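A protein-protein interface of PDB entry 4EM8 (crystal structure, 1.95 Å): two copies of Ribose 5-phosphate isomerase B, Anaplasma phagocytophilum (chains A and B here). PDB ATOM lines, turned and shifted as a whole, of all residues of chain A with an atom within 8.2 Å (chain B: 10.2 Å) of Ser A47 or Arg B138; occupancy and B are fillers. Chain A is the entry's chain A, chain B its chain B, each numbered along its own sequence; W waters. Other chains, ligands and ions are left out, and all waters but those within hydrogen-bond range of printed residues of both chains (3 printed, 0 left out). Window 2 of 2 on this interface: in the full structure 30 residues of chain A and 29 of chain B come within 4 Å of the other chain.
The side-chain carboxylate (OD1) of Asp A49 is in salt-bridge range of the guanidinium group (NE) of Arg B142 (3.1 Å).
OG of Ser A47 lies within hydrogen-bond range of NH2 of Arg B138 (2.8 Å).
NH2 of Arg B142 is in hydrogen-bond range of O of Val A48.
OD2 of Asp A49 lies within salt-bridge range of NZ of Lys B145, at 2.6 Å.
ND2 of Asn B105 is in hydrogen-bond range of OH of Tyr A50 (2.9 Å).
A ring nitrogen (ND1) of His A16 sits at hydrogen-bond distance from the backbone NH of Val A48 (3.1 Å).
The backbone NH of His A16 lies within hydrogen-bond range of the side-chain sulfur of Cys A41.
CE1 of His A16 touches NH2 of Arg B142 (3.7 Å).
Ser A47 touches Arg B142 (OG to NH2, 3.5 Å).
Val B141 touches Asp A49.
Arg B142 touches Tyr A50 (CB to CE2, 3.7 Å).
Ser A47 touches just these residues of chain B: Arg B138 (2.8 Å) and Arg B142 (3.5 Å).
Val A48 touches just one residue of chain B: Arg B142 (3.4 Å).
No residue of chain A comes within 4 Å of Gly B137.
Of the printed residues of chain A, Asn B105 touches Tyr A50 (2.9 Å).
Of the printed residues of chain A, Val B141 touches Asp A49.
Asp A42 touches none of the printed residues of chain B.
Pro A43 touches none of the printed residues of chain B.
The nearest residue of chain B that does not touch Ser A47 is Val B141 (8.0 Å).
Printed residues of chain A that touch a printed residue of chain B: His A16, Ser A47, Val A48, Asp A49 and Tyr A50.
No position is printed for both chains.
Of the 9 pairs that touch across the chains among the printed residues, none has its exchanged pair printed and touching as well.
Water W2 lies within hydrogen-bond range of the side-chain hydroxyl (OH) of Tyr A50 (2.6 Å) and the backbone carbonyl oxygen (O) of His B104 (2.8 Å).
Water W3 lies within hydrogen-bond range of O of Val A48 (2.7 Å), OD2 of Asp A15 (2.8 Å), N of Tyr A50 (2.9 Å) and NE of Arg B142 (3.2 Å).
Water W1 bridges OD1 of Asp A49 (2.8 Å) and NH2 of Arg B142 (3.2 Å).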
ATOM      1  N   ASP A  15      10.122  13.255  -8.430  1.00  0.00           N
ATOM      2  CA  ASP A  15      10.326  12.705  -7.113  1.00  0.00           C
ATOM      3  C   ASP A  15      10.121  11.193  -7.221  1.00  0.00           C
ATOM      4  O   ASP A  15      10.022  10.630  -8.328  1.00  0.00           O
ATOM      5  CB  ASP A  15       9.450  13.408  -6.041  1.00  0.00           C
ATOM      6  CG  ASP A  15       7.989  13.074  -6.134  1.00  0.00           C
ATOM      7  OD1 ASP A  15       7.585  12.300  -7.013  1.00  0.00           O
ATOM      8  OD2 ASP A  15       7.218  13.615  -5.306  1.00  0.00           O
ATOM      9  N   HIS A  16      10.106  10.526  -6.085  1.00  0.00           N
ATOM     10  CA  HIS A  16      10.057   9.070  -6.084  1.00  0.00           C
ATOM     11  C   HIS A  16       8.798   8.559  -6.729  1.00  0.00           C
ATOM     12  O   HIS A  16       8.826   7.513  -7.356  1.00  0.00           O
ATOM     13  CB  HIS A  16      10.125   8.558  -4.651  1.00  0.00           C
ATOM     14  CG  HIS A  16       9.158   9.237  -3.747  1.00  0.00           C
ATOM     15  ND1 HIS A  16       9.341  10.496  -3.307  1.00  0.00           N
ATOM     16  CD2 HIS A  16       7.945   8.808  -3.221  1.00  0.00           C
ATOM     17  CE1 HIS A  16       8.312  10.848  -2.513  1.00  0.00           C
ATOM     18  NE2 HIS A  16       7.454   9.822  -2.470  1.00  0.00           N
ATOM     19  N   ALA A  17       7.688   9.291  -6.582  1.00  0.00           N
ATOM     20  CA  ALA A  17       6.387   8.849  -7.124  1.00  0.00           C
ATOM     21  C   ALA A  17       6.415   8.811  -8.650  1.00  0.00           C
ATOM     22  O   ALA A  17       5.768   7.974  -9.285  1.00  0.00           O
ATOM     23  CB  ALA A  17       5.260   9.783  -6.649  1.00  0.00           C
ATOM     24  N   CYS A  41      14.824  12.261  -9.770  1.00  0.00           N
ATOM     25  CA  CYS A  41      15.715  11.645  -8.755  1.00  0.00           C
ATOM     26  C   CYS A  41      16.213  10.273  -9.164  1.00  0.00           C
ATOM     27  O   CYS A  41      15.684   9.636 -10.076  1.00  0.00           O
ATOM     28  CB  CYS A  41      14.988  11.512  -7.428  1.00  0.00           C
ATOM     29  SG  CYS A  41      13.553  10.411  -7.522  1.00  0.00           S
ATOM     30  N   ASP A  42      17.228   9.813  -8.461  1.00  0.00           N
ATOM     31  CA  ASP A  42      17.797   8.496  -8.690  1.00  0.00           C
ATOM     32  C   ASP A  42      16.680   7.484  -8.428  1.00  0.00           C
ATOM     33  O   ASP A  42      16.006   7.574  -7.399  1.00  0.00           O
ATOM     34  CB  ASP A  42      18.953   8.312  -7.706  1.00  0.00           C
ATOM     35  CG  ASP A  42      19.717   7.009  -7.890  1.00  0.00           C
ATOM     36  OD1 ASP A  42      19.142   5.950  -8.204  1.00  0.00           O
ATOM     37  OD2 ASP A  42      20.936   7.052  -7.653  1.00  0.00           O
ATOM     38  N   PRO A  43      16.468   6.528  -9.343  1.00  0.00           N
ATOM     39  CA  PRO A  43      15.424   5.507  -9.105  1.00  0.00           C
ATOM     40  C   PRO A  43      15.577   4.705  -7.807  1.00  0.00           C
ATOM     41  O   PRO A  43      14.584   4.241  -7.273  1.00  0.00           O
ATOM     42  CB  PRO A  43      15.539   4.578 -10.318  1.00  0.00           C
ATOM     43  CG  PRO A  43      16.180   5.412 -11.381  1.00  0.00           C
ATOM     44  CD  PRO A  43      17.079   6.401 -10.676  1.00  0.00           C
ATOM     45  N   LYS A  44      16.799   4.562  -7.302  1.00  0.00           N
ATOM     46  CA  LYS A  44      17.053   3.909  -6.003  1.00  0.00           C
ATOM     47  C   LYS A  44      16.415   4.661  -4.817  1.00  0.00           C
ATOM     48  O   LYS A  44      16.298   4.111  -3.735  1.00  0.00           O
ATOM     49  CB  LYS A  44      18.568   3.750  -5.770  1.00  0.00           C
ATOM     50  N   GLU A  45      16.030   5.920  -5.019  1.00  0.00           N
ATOM     51  CA  GLU A  45      15.470   6.743  -3.943  1.00  0.00           C
ATOM     52  C   GLU A  45      13.979   6.456  -3.784  1.00  0.00           C
ATOM     53  O   GLU A  45      13.190   6.664  -4.725  1.00  0.00           O
ATOM     54  CB  GLU A  45      15.670   8.249  -4.230  1.00  0.00           C
ATOM     55  CG  GLU A  45      17.103   8.773  -4.123  1.00  0.00           C
ATOM     56  CD  GLU A  45      17.620   8.813  -2.693  1.00  0.00           C
ATOM     57  OE1 GLU A  45      16.986   9.471  -1.842  1.00  0.00           O
ATOM     58  OE2 GLU A  45      18.671   8.181  -2.417  1.00  0.00           O
ATOM     59  N   HIS A  46      13.591   6.036  -2.585  1.00  0.00           N
ATOM     60  CA  HIS A  46      12.187   5.704  -2.297  1.00  0.00           C
ATOM     61  C   HIS A  46      11.387   6.827  -1.666  1.00  0.00           C
ATOM     62  O   HIS A  46      10.166   6.770  -1.667  1.00  0.00           O
ATOM     63  CB  HIS A  46      12.107   4.405  -1.487  1.00  0.00           C
ATOM     64  CG  HIS A  46      12.330   3.153  -2.325  1.00  0.00           C
ATOM     65  ND1 HIS A  46      13.179   3.122  -3.394  1.00  0.00           N
ATOM     66  CD2 HIS A  46      11.793   1.866  -2.211  1.00  0.00           C
ATOM     67  CE1 HIS A  46      13.175   1.880  -3.933  1.00  0.00           C
ATOM     68  NE2 HIS A  46      12.329   1.111  -3.207  1.00  0.00           N
ATOM     69  N   SER A  47      12.048   7.850  -1.128  1.00  0.00           N
ATOM     70  CA  SER A  47      11.371   9.089  -0.738  1.00  0.00           C
ATOM     71  C   SER A  47      12.255  10.337  -0.871  1.00  0.00           C
ATOM     72  O   SER A  47      13.272  10.441  -0.203  1.00  0.00           O
ATOM     73  CB  SER A  47      10.836   9.001   0.698  1.00  0.00           C
ATOM     74  OG  SER A  47       9.999  10.120   0.934  1.00  0.00           O
ATOM     75  N   VAL A  48      11.864  11.284  -1.735  1.00  0.00           N
ATOM     76  CA  VAL A  48      12.513  12.594  -1.823  1.00  0.00           C
ATOM     77  C   VAL A  48      11.463  13.713  -1.865  1.00  0.00           C
ATOM     78  O   VAL A  48      10.280  13.432  -1.883  1.00  0.00           O
ATOM     79  CB  VAL A  48      13.421  12.709  -3.078  1.00  0.00           C
ATOM     80  CG1 VAL A  48      14.613  11.759  -2.968  1.00  0.00           C
ATOM     81  CG2 VAL A  48      12.600  12.482  -4.351  1.00  0.00           C
ATOM     82  N   ASP A  49      11.920  14.971  -1.849  1.00  0.00           N
ATOM     83  CA  ASP A  49      11.049  16.144  -1.851  1.00  0.00           C
ATOM     84  C   ASP A  49      11.003  16.778  -3.255  1.00  0.00           C
ATOM     85  O   ASP A  49      12.030  17.247  -3.762  1.00  0.00           O
ATOM     86  CB  ASP A  49      11.546  17.171  -0.815  1.00  0.00           C
ATOM     87  CG  ASP A  49      11.446  16.665   0.620  1.00  0.00           C
ATOM     88  OD1 ASP A  49      10.645  15.752   0.914  1.00  0.00           O
ATOM     89  OD2 ASP A  49      12.173  17.208   1.447  1.00  0.00           O
ATOM     90  N   TYR A  50       9.829  16.779  -3.891  1.00  0.00           N
ATOM     91  CA  TYR A  50       9.721  17.268  -5.278  1.00  0.00           C
ATOM     92  C   TYR A  50      10.361  18.639  -5.494  1.00  0.00           C
ATOM     93  O   TYR A  50      10.998  18.853  -6.527  1.00  0.00           O
ATOM     94  CB  TYR A  50       8.266  17.194  -5.829  1.00  0.00           C
ATOM     95  CG  TYR A  50       7.248  17.950  -5.010  1.00  0.00           C
ATOM     96  CD1 TYR A  50       6.999  19.295  -5.250  1.00  0.00           C
ATOM     97  CD2 TYR A  50       6.550  17.325  -3.978  1.00  0.00           C
ATOM     98  CE1 TYR A  50       6.085  20.003  -4.476  1.00  0.00           C
ATOM     99  CE2 TYR A  50       5.618  18.023  -3.199  1.00  0.00           C
ATOM    100  CZ  TYR A  50       5.404  19.361  -3.438  1.00  0.00           C
ATOM    101  OH  TYR A  50       4.492  20.054  -2.671  1.00  0.00           O
ATOM    102  N   TYR A  53      13.967  18.868  -6.937  1.00  0.00           N
ATOM    103  CA  TYR A  53      14.258  18.336  -8.286  1.00  0.00           C
ATOM    104  C   TYR A  53      13.786  19.238  -9.451  1.00  0.00           C
ATOM    105  O   TYR A  53      13.848  18.874 -10.627  1.00  0.00           O
ATOM    106  CB  TYR A  53      13.740  16.893  -8.361  1.00  0.00           C
ATOM    107  CG  TYR A  53      14.614  16.004  -7.510  1.00  0.00           C
ATOM    108  CD1 TYR A  53      14.380  15.878  -6.145  1.00  0.00           C
ATOM    109  CD2 TYR A  53      15.712  15.367  -8.053  1.00  0.00           C
ATOM    110  CE1 TYR A  53      15.199  15.102  -5.354  1.00  0.00           C
ATOM    111  CE2 TYR A  53      16.544  14.592  -7.273  1.00  0.00           C
ATOM    112  CZ  TYR A  53      16.264  14.459  -5.923  1.00  0.00           C
ATOM    113  OH  TYR A  53      17.067  13.716  -5.127  1.00  0.00           O
ATOM    114  N   ARG A 115       0.403   9.433 -10.142  1.00  0.00           N
ATOM    115  CA  ARG A 115      -0.578   8.572  -9.489  1.00  0.00           C
ATOM    116  C   ARG A 115      -1.996   8.683 -10.033  1.00  0.00           C
ATOM    117  O   ARG A 115      -2.845   7.937  -9.621  1.00  0.00           O
ATOM    118  CB  ARG A 115      -0.561   8.819  -7.967  1.00  0.00           C
ATOM    119  CG  ARG A 115       0.710   8.290  -7.352  1.00  0.00           C
ATOM    120  CD  ARG A 115       0.814   8.575  -5.878  1.00  0.00           C
ATOM    121  NE  ARG A 115       2.043   7.990  -5.321  1.00  0.00           N
ATOM    122  CZ  ARG A 115       2.680   8.437  -4.235  1.00  0.00           C
ATOM    123  NH1 ARG A 115       2.216   9.474  -3.563  1.00  0.00           N
ATOM    124  NH2 ARG A 115       3.784   7.829  -3.811  1.00  0.00           N
ATOM    125  N   GLU B 103      -4.898  19.276   0.818  1.00  0.00           N
ATOM    126  CA  GLU B 103      -4.273  18.245   1.657  1.00  0.00           C
ATOM    127  C   GLU B 103      -2.744  18.179   1.541  1.00  0.00           C
ATOM    128  O   GLU B 103      -2.041  18.120   2.569  1.00  0.00           O
ATOM    129  CB  GLU B 103      -4.868  16.854   1.364  1.00  0.00           C
ATOM    130  CG  GLU B 103      -6.291  16.735   1.847  1.00  0.00           C
ATOM    131  CD  GLU B 103      -6.880  15.356   1.640  1.00  0.00           C
ATOM    132  OE1 GLU B 103      -6.551  14.664   0.657  1.00  0.00           O
ATOM    133  OE2 GLU B 103      -7.711  15.000   2.472  1.00  0.00           O
ATOM    134  N   HIS B 104      -2.230  18.172   0.308  1.00  0.00           N
ATOM    135  CA  HIS B 104      -0.801  17.939   0.088  1.00  0.00           C
ATOM    136  C   HIS B 104      -0.012  19.237   0.036  1.00  0.00           C
ATOM    137  O   HIS B 104       1.103  19.317   0.527  1.00  0.00           O
ATOM    138  CB  HIS B 104      -0.551  17.154  -1.209  1.00  0.00           C
ATOM    139  CG  HIS B 104      -1.289  15.832  -1.307  1.00  0.00           C
ATOM    140  ND1 HIS B 104      -1.979  15.271  -0.259  1.00  0.00           N
ATOM    141  CD2 HIS B 104      -1.385  14.930  -2.357  1.00  0.00           C
ATOM    142  CE1 HIS B 104      -2.500  14.091  -0.653  1.00  0.00           C
ATOM    143  NE2 HIS B 104      -2.135  13.879  -1.926  1.00  0.00           N
ATOM    144  N   ASN B 105      -0.569  20.267  -0.598  1.00  0.00           N
ATOM    145  CA  ASN B 105       0.192  21.493  -0.865  1.00  0.00           C
ATOM    146  C   ASN B 105      -0.265  22.717  -0.079  1.00  0.00           C
ATOM    147  O   ASN B 105       0.306  23.811  -0.271  1.00  0.00           O
ATOM    148  CB  ASN B 105       0.169  21.772  -2.373  1.00  0.00           C
ATOM    149  CG  ASN B 105       0.413  20.511  -3.183  1.00  0.00           C
ATOM    150  OD1 ASN B 105      -0.529  19.830  -3.559  1.00  0.00           O
ATOM    151  ND2 ASN B 105       1.679  20.170  -3.398  1.00  0.00           N
ATOM    152  N   PHE B 134      -5.222  21.067   5.499  1.00  0.00           N
ATOM    153  CA  PHE B 134      -3.894  20.622   5.125  1.00  0.00           C
ATOM    154  C   PHE B 134      -3.521  19.449   6.009  1.00  0.00           C
ATOM    155  O   PHE B 134      -3.737  19.488   7.202  1.00  0.00           O
ATOM    156  CB  PHE B 134      -2.914  21.778   5.356  1.00  0.00           C
ATOM    157  CG  PHE B 134      -1.461  21.450   5.076  1.00  0.00           C
ATOM    158  CD1 PHE B 134      -1.078  20.805   3.905  1.00  0.00           C
ATOM    159  CD2 PHE B 134      -0.464  21.837   5.976  1.00  0.00           C
ATOM    160  CE1 PHE B 134       0.254  20.515   3.659  1.00  0.00           C
ATOM    161  CE2 PHE B 134       0.874  21.583   5.712  1.00  0.00           C
ATOM    162  CZ  PHE B 134       1.235  20.913   4.550  1.00  0.00           C
ATOM    163  N   LEU B 135      -2.933  18.418   5.421  1.00  0.00           N
ATOM    164  CA  LEU B 135      -2.565  17.233   6.172  1.00  0.00           C
ATOM    165  C   LEU B 135      -1.258  17.392   6.939  1.00  0.00           C
ATOM    166  O   LEU B 135      -1.042  16.703   7.921  1.00  0.00           O
ATOM    167  CB  LEU B 135      -2.515  16.014   5.249  1.00  0.00           C
ATOM    168  CG  LEU B 135      -3.878  15.603   4.696  1.00  0.00           C
ATOM    169  CD1 LEU B 135      -3.773  14.339   3.849  1.00  0.00           C
ATOM    170  CD2 LEU B 135      -4.880  15.434   5.830  1.00  0.00           C
ATOM    171  N   GLY B 136      -0.395  18.313   6.536  1.00  0.00           N
ATOM    172  CA  GLY B 136       0.924  18.412   7.182  1.00  0.00           C
ATOM    173  C   GLY B 136       1.679  17.094   7.078  1.00  0.00           C
ATOM    174  O   GLY B 136       1.712  16.463   6.008  1.00  0.00           O
ATOM    175  N   GLY B 137       2.255  16.651   8.198  1.00  0.00           N
ATOM    176  CA  GLY B 137       3.066  15.436   8.210  1.00  0.00           C
ATOM    177  C   GLY B 137       4.229  15.459   7.229  1.00  0.00           C
ATOM    178  O   GLY B 137       5.075  16.374   7.240  1.00  0.00           O
ATOM    179  N   ARG B 138       4.277  14.462   6.351  1.00  0.00           N
ATOM    180  CA  ARG B 138       5.370  14.377   5.358  1.00  0.00           C
ATOM    181  C   ARG B 138       5.310  15.480   4.280  1.00  0.00           C
ATOM    182  O   ARG B 138       6.324  15.810   3.641  1.00  0.00           O
ATOM    183  CB  ARG B 138       5.386  12.984   4.735  1.00  0.00           C
ATOM    184  CG  ARG B 138       5.741  11.905   5.773  1.00  0.00           C
ATOM    185  CD  ARG B 138       5.957  10.526   5.186  1.00  0.00           C
ATOM    186  NE  ARG B 138       7.084  10.456   4.265  1.00  0.00           N
ATOM    187  CZ  ARG B 138       8.369  10.343   4.595  1.00  0.00           C
ATOM    188  NH1 ARG B 138       8.769  10.279   5.860  1.00  0.00           N
ATOM    189  NH2 ARG B 138       9.280  10.282   3.625  1.00  0.00           N
ATOM    190  N   HIS B 139       4.131  16.079   4.121  1.00  0.00           N
ATOM    191  CA  HIS B 139       3.961  17.209   3.207  1.00  0.00           C
ATOM    192  C   HIS B 139       4.536  18.503   3.723  1.00  0.00           C
ATOM    193  O   HIS B 139       4.892  19.380   2.923  1.00  0.00           O
ATOM    194  CB  HIS B 139       2.497  17.406   2.872  1.00  0.00           C
ATOM    195  CG  HIS B 139       1.787  16.134   2.467  1.00  0.00           C
ATOM    196  ND1 HIS B 139       2.006  15.523   1.280  1.00  0.00           N
ATOM    197  CD2 HIS B 139       0.842  15.373   3.130  1.00  0.00           C
ATOM    198  CE1 HIS B 139       1.229  14.430   1.196  1.00  0.00           C
ATOM    199  NE2 HIS B 139       0.528  14.334   2.336  1.00  0.00           N
ATOM    200  N   ALA B 140       4.654  18.633   5.052  1.00  0.00           N
ATOM    201  CA  ALA B 140       5.040  19.898   5.670  1.00  0.00           C
ATOM    202  C   ALA B 140       6.365  20.342   5.120  1.00  0.00           C
ATOM    203  O   ALA B 140       6.521  21.485   4.701  1.00  0.00           O
ATOM    204  CB  ALA B 140       5.111  19.768   7.194  1.00  0.00           C
ATOM    205  N   VAL B 141       7.327  19.426   5.089  1.00  0.00           N
ATOM    206  CA  VAL B 141       8.665  19.806   4.644  1.00  0.00           C
ATOM    207  C   VAL B 141       8.643  20.286   3.194  1.00  0.00           C
ATOM    208  O   VAL B 141       9.323  21.240   2.850  1.00  0.00           O
ATOM    209  CB  VAL B 141       9.702  18.687   4.847  1.00  0.00           C
ATOM    210  CG1 VAL B 141       9.361  17.445   4.036  1.00  0.00           C
ATOM    211  CG2 VAL B 141      11.095  19.205   4.497  1.00  0.00           C
ATOM    212  N   ARG B 142       7.839  19.650   2.349  1.00  0.00           N
ATOM    213  CA  ARG B 142       7.795  20.060   0.927  1.00  0.00           C
ATOM    214  C   ARG B 142       7.141  21.440   0.778  1.00  0.00           C
ATOM    215  O   ARG B 142       7.634  22.300   0.027  1.00  0.00           O
ATOM    216  CB  ARG B 142       7.101  18.992   0.083  1.00  0.00           C
ATOM    217  CG  ARG B 142       7.817  17.643   0.172  1.00  0.00           C
ATOM    218  CD  ARG B 142       6.889  16.436   0.025  1.00  0.00           C
ATOM    219  NE  ARG B 142       7.656  15.223   0.249  1.00  0.00           N
ATOM    220  CZ  ARG B 142       7.158  13.996   0.317  1.00  0.00           C
ATOM    221  NH1 ARG B 142       5.862  13.784   0.149  1.00  0.00           N
ATOM    222  NH2 ARG B 142       7.969  12.976   0.531  1.00  0.00           N
ATOM    223  N   VAL B 143       6.068  21.665   1.536  1.00  0.00           N
ATOM    224  CA  VAL B 143       5.365  22.956   1.530  1.00  0.00           C
ATOM    225  C   VAL B 143       6.320  24.050   2.007  1.00  0.00           C
ATOM    226  O   VAL B 143       6.343  25.134   1.417  1.00  0.00           O
ATOM    227  CB  VAL B 143       4.046  22.902   2.340  1.00  0.00           C
ATOM    228  CG1 VAL B 143       3.403  24.273   2.446  1.00  0.00           C
ATOM    229  CG2 VAL B 143       3.078  21.931   1.667  1.00  0.00           C
ATOM    230  N   GLN B 144       7.131  23.765   3.034  1.00  0.00           N
ATOM    231  CA  GLN B 144       8.154  24.727   3.524  1.00  0.00           C
ATOM    232  C   GLN B 144       9.118  25.082   2.425  1.00  0.00           C
ATOM    233  O   GLN B 144       9.502  26.254   2.247  1.00  0.00           O
ATOM    234  CB  GLN B 144       9.024  24.130   4.633  1.00  0.00           C
ATOM    235  CG  GLN B 144       8.408  23.971   6.006  1.00  0.00           C
ATOM    236  CD  GLN B 144       9.424  23.433   6.998  1.00  0.00           C
ATOM    237  OE1 GLN B 144       9.354  22.264   7.439  1.00  0.00           O
ATOM    238  NE2 GLN B 144      10.414  24.266   7.318  1.00  0.00           N
ATOM    239  N   LYS B 145       9.574  24.041   1.727  1.00  0.00           N
ATOM    240  CA  LYS B 145      10.513  24.232   0.627  1.00  0.00           C
ATOM    241  C   LYS B 145       9.913  25.053  -0.513  1.00  0.00           C
ATOM    242  O   LYS B 145      10.607  25.852  -1.115  1.00  0.00           O
ATOM    243  CB  LYS B 145      11.044  22.893   0.131  1.00  0.00           C
ATOM    244  CG  LYS B 145      11.983  22.190   1.126  1.00  0.00           C
ATOM    245  CD  LYS B 145      12.586  20.930   0.527  1.00  0.00           C
ATOM    246  CE  LYS B 145      13.817  20.452   1.320  1.00  0.00           C
ATOM    247  NZ  LYS B 145      14.015  18.975   1.215  1.00  0.00           N
HETATM  248  O   HOH W   1      10.550  13.442   2.424  1.00  0.00           O
HETATM  249  O   HOH W   2       3.543  18.747  -0.609  1.00  0.00           O
HETATM  250  O   HOH W   3       8.079  14.646  -2.876  1.00  0.00           O
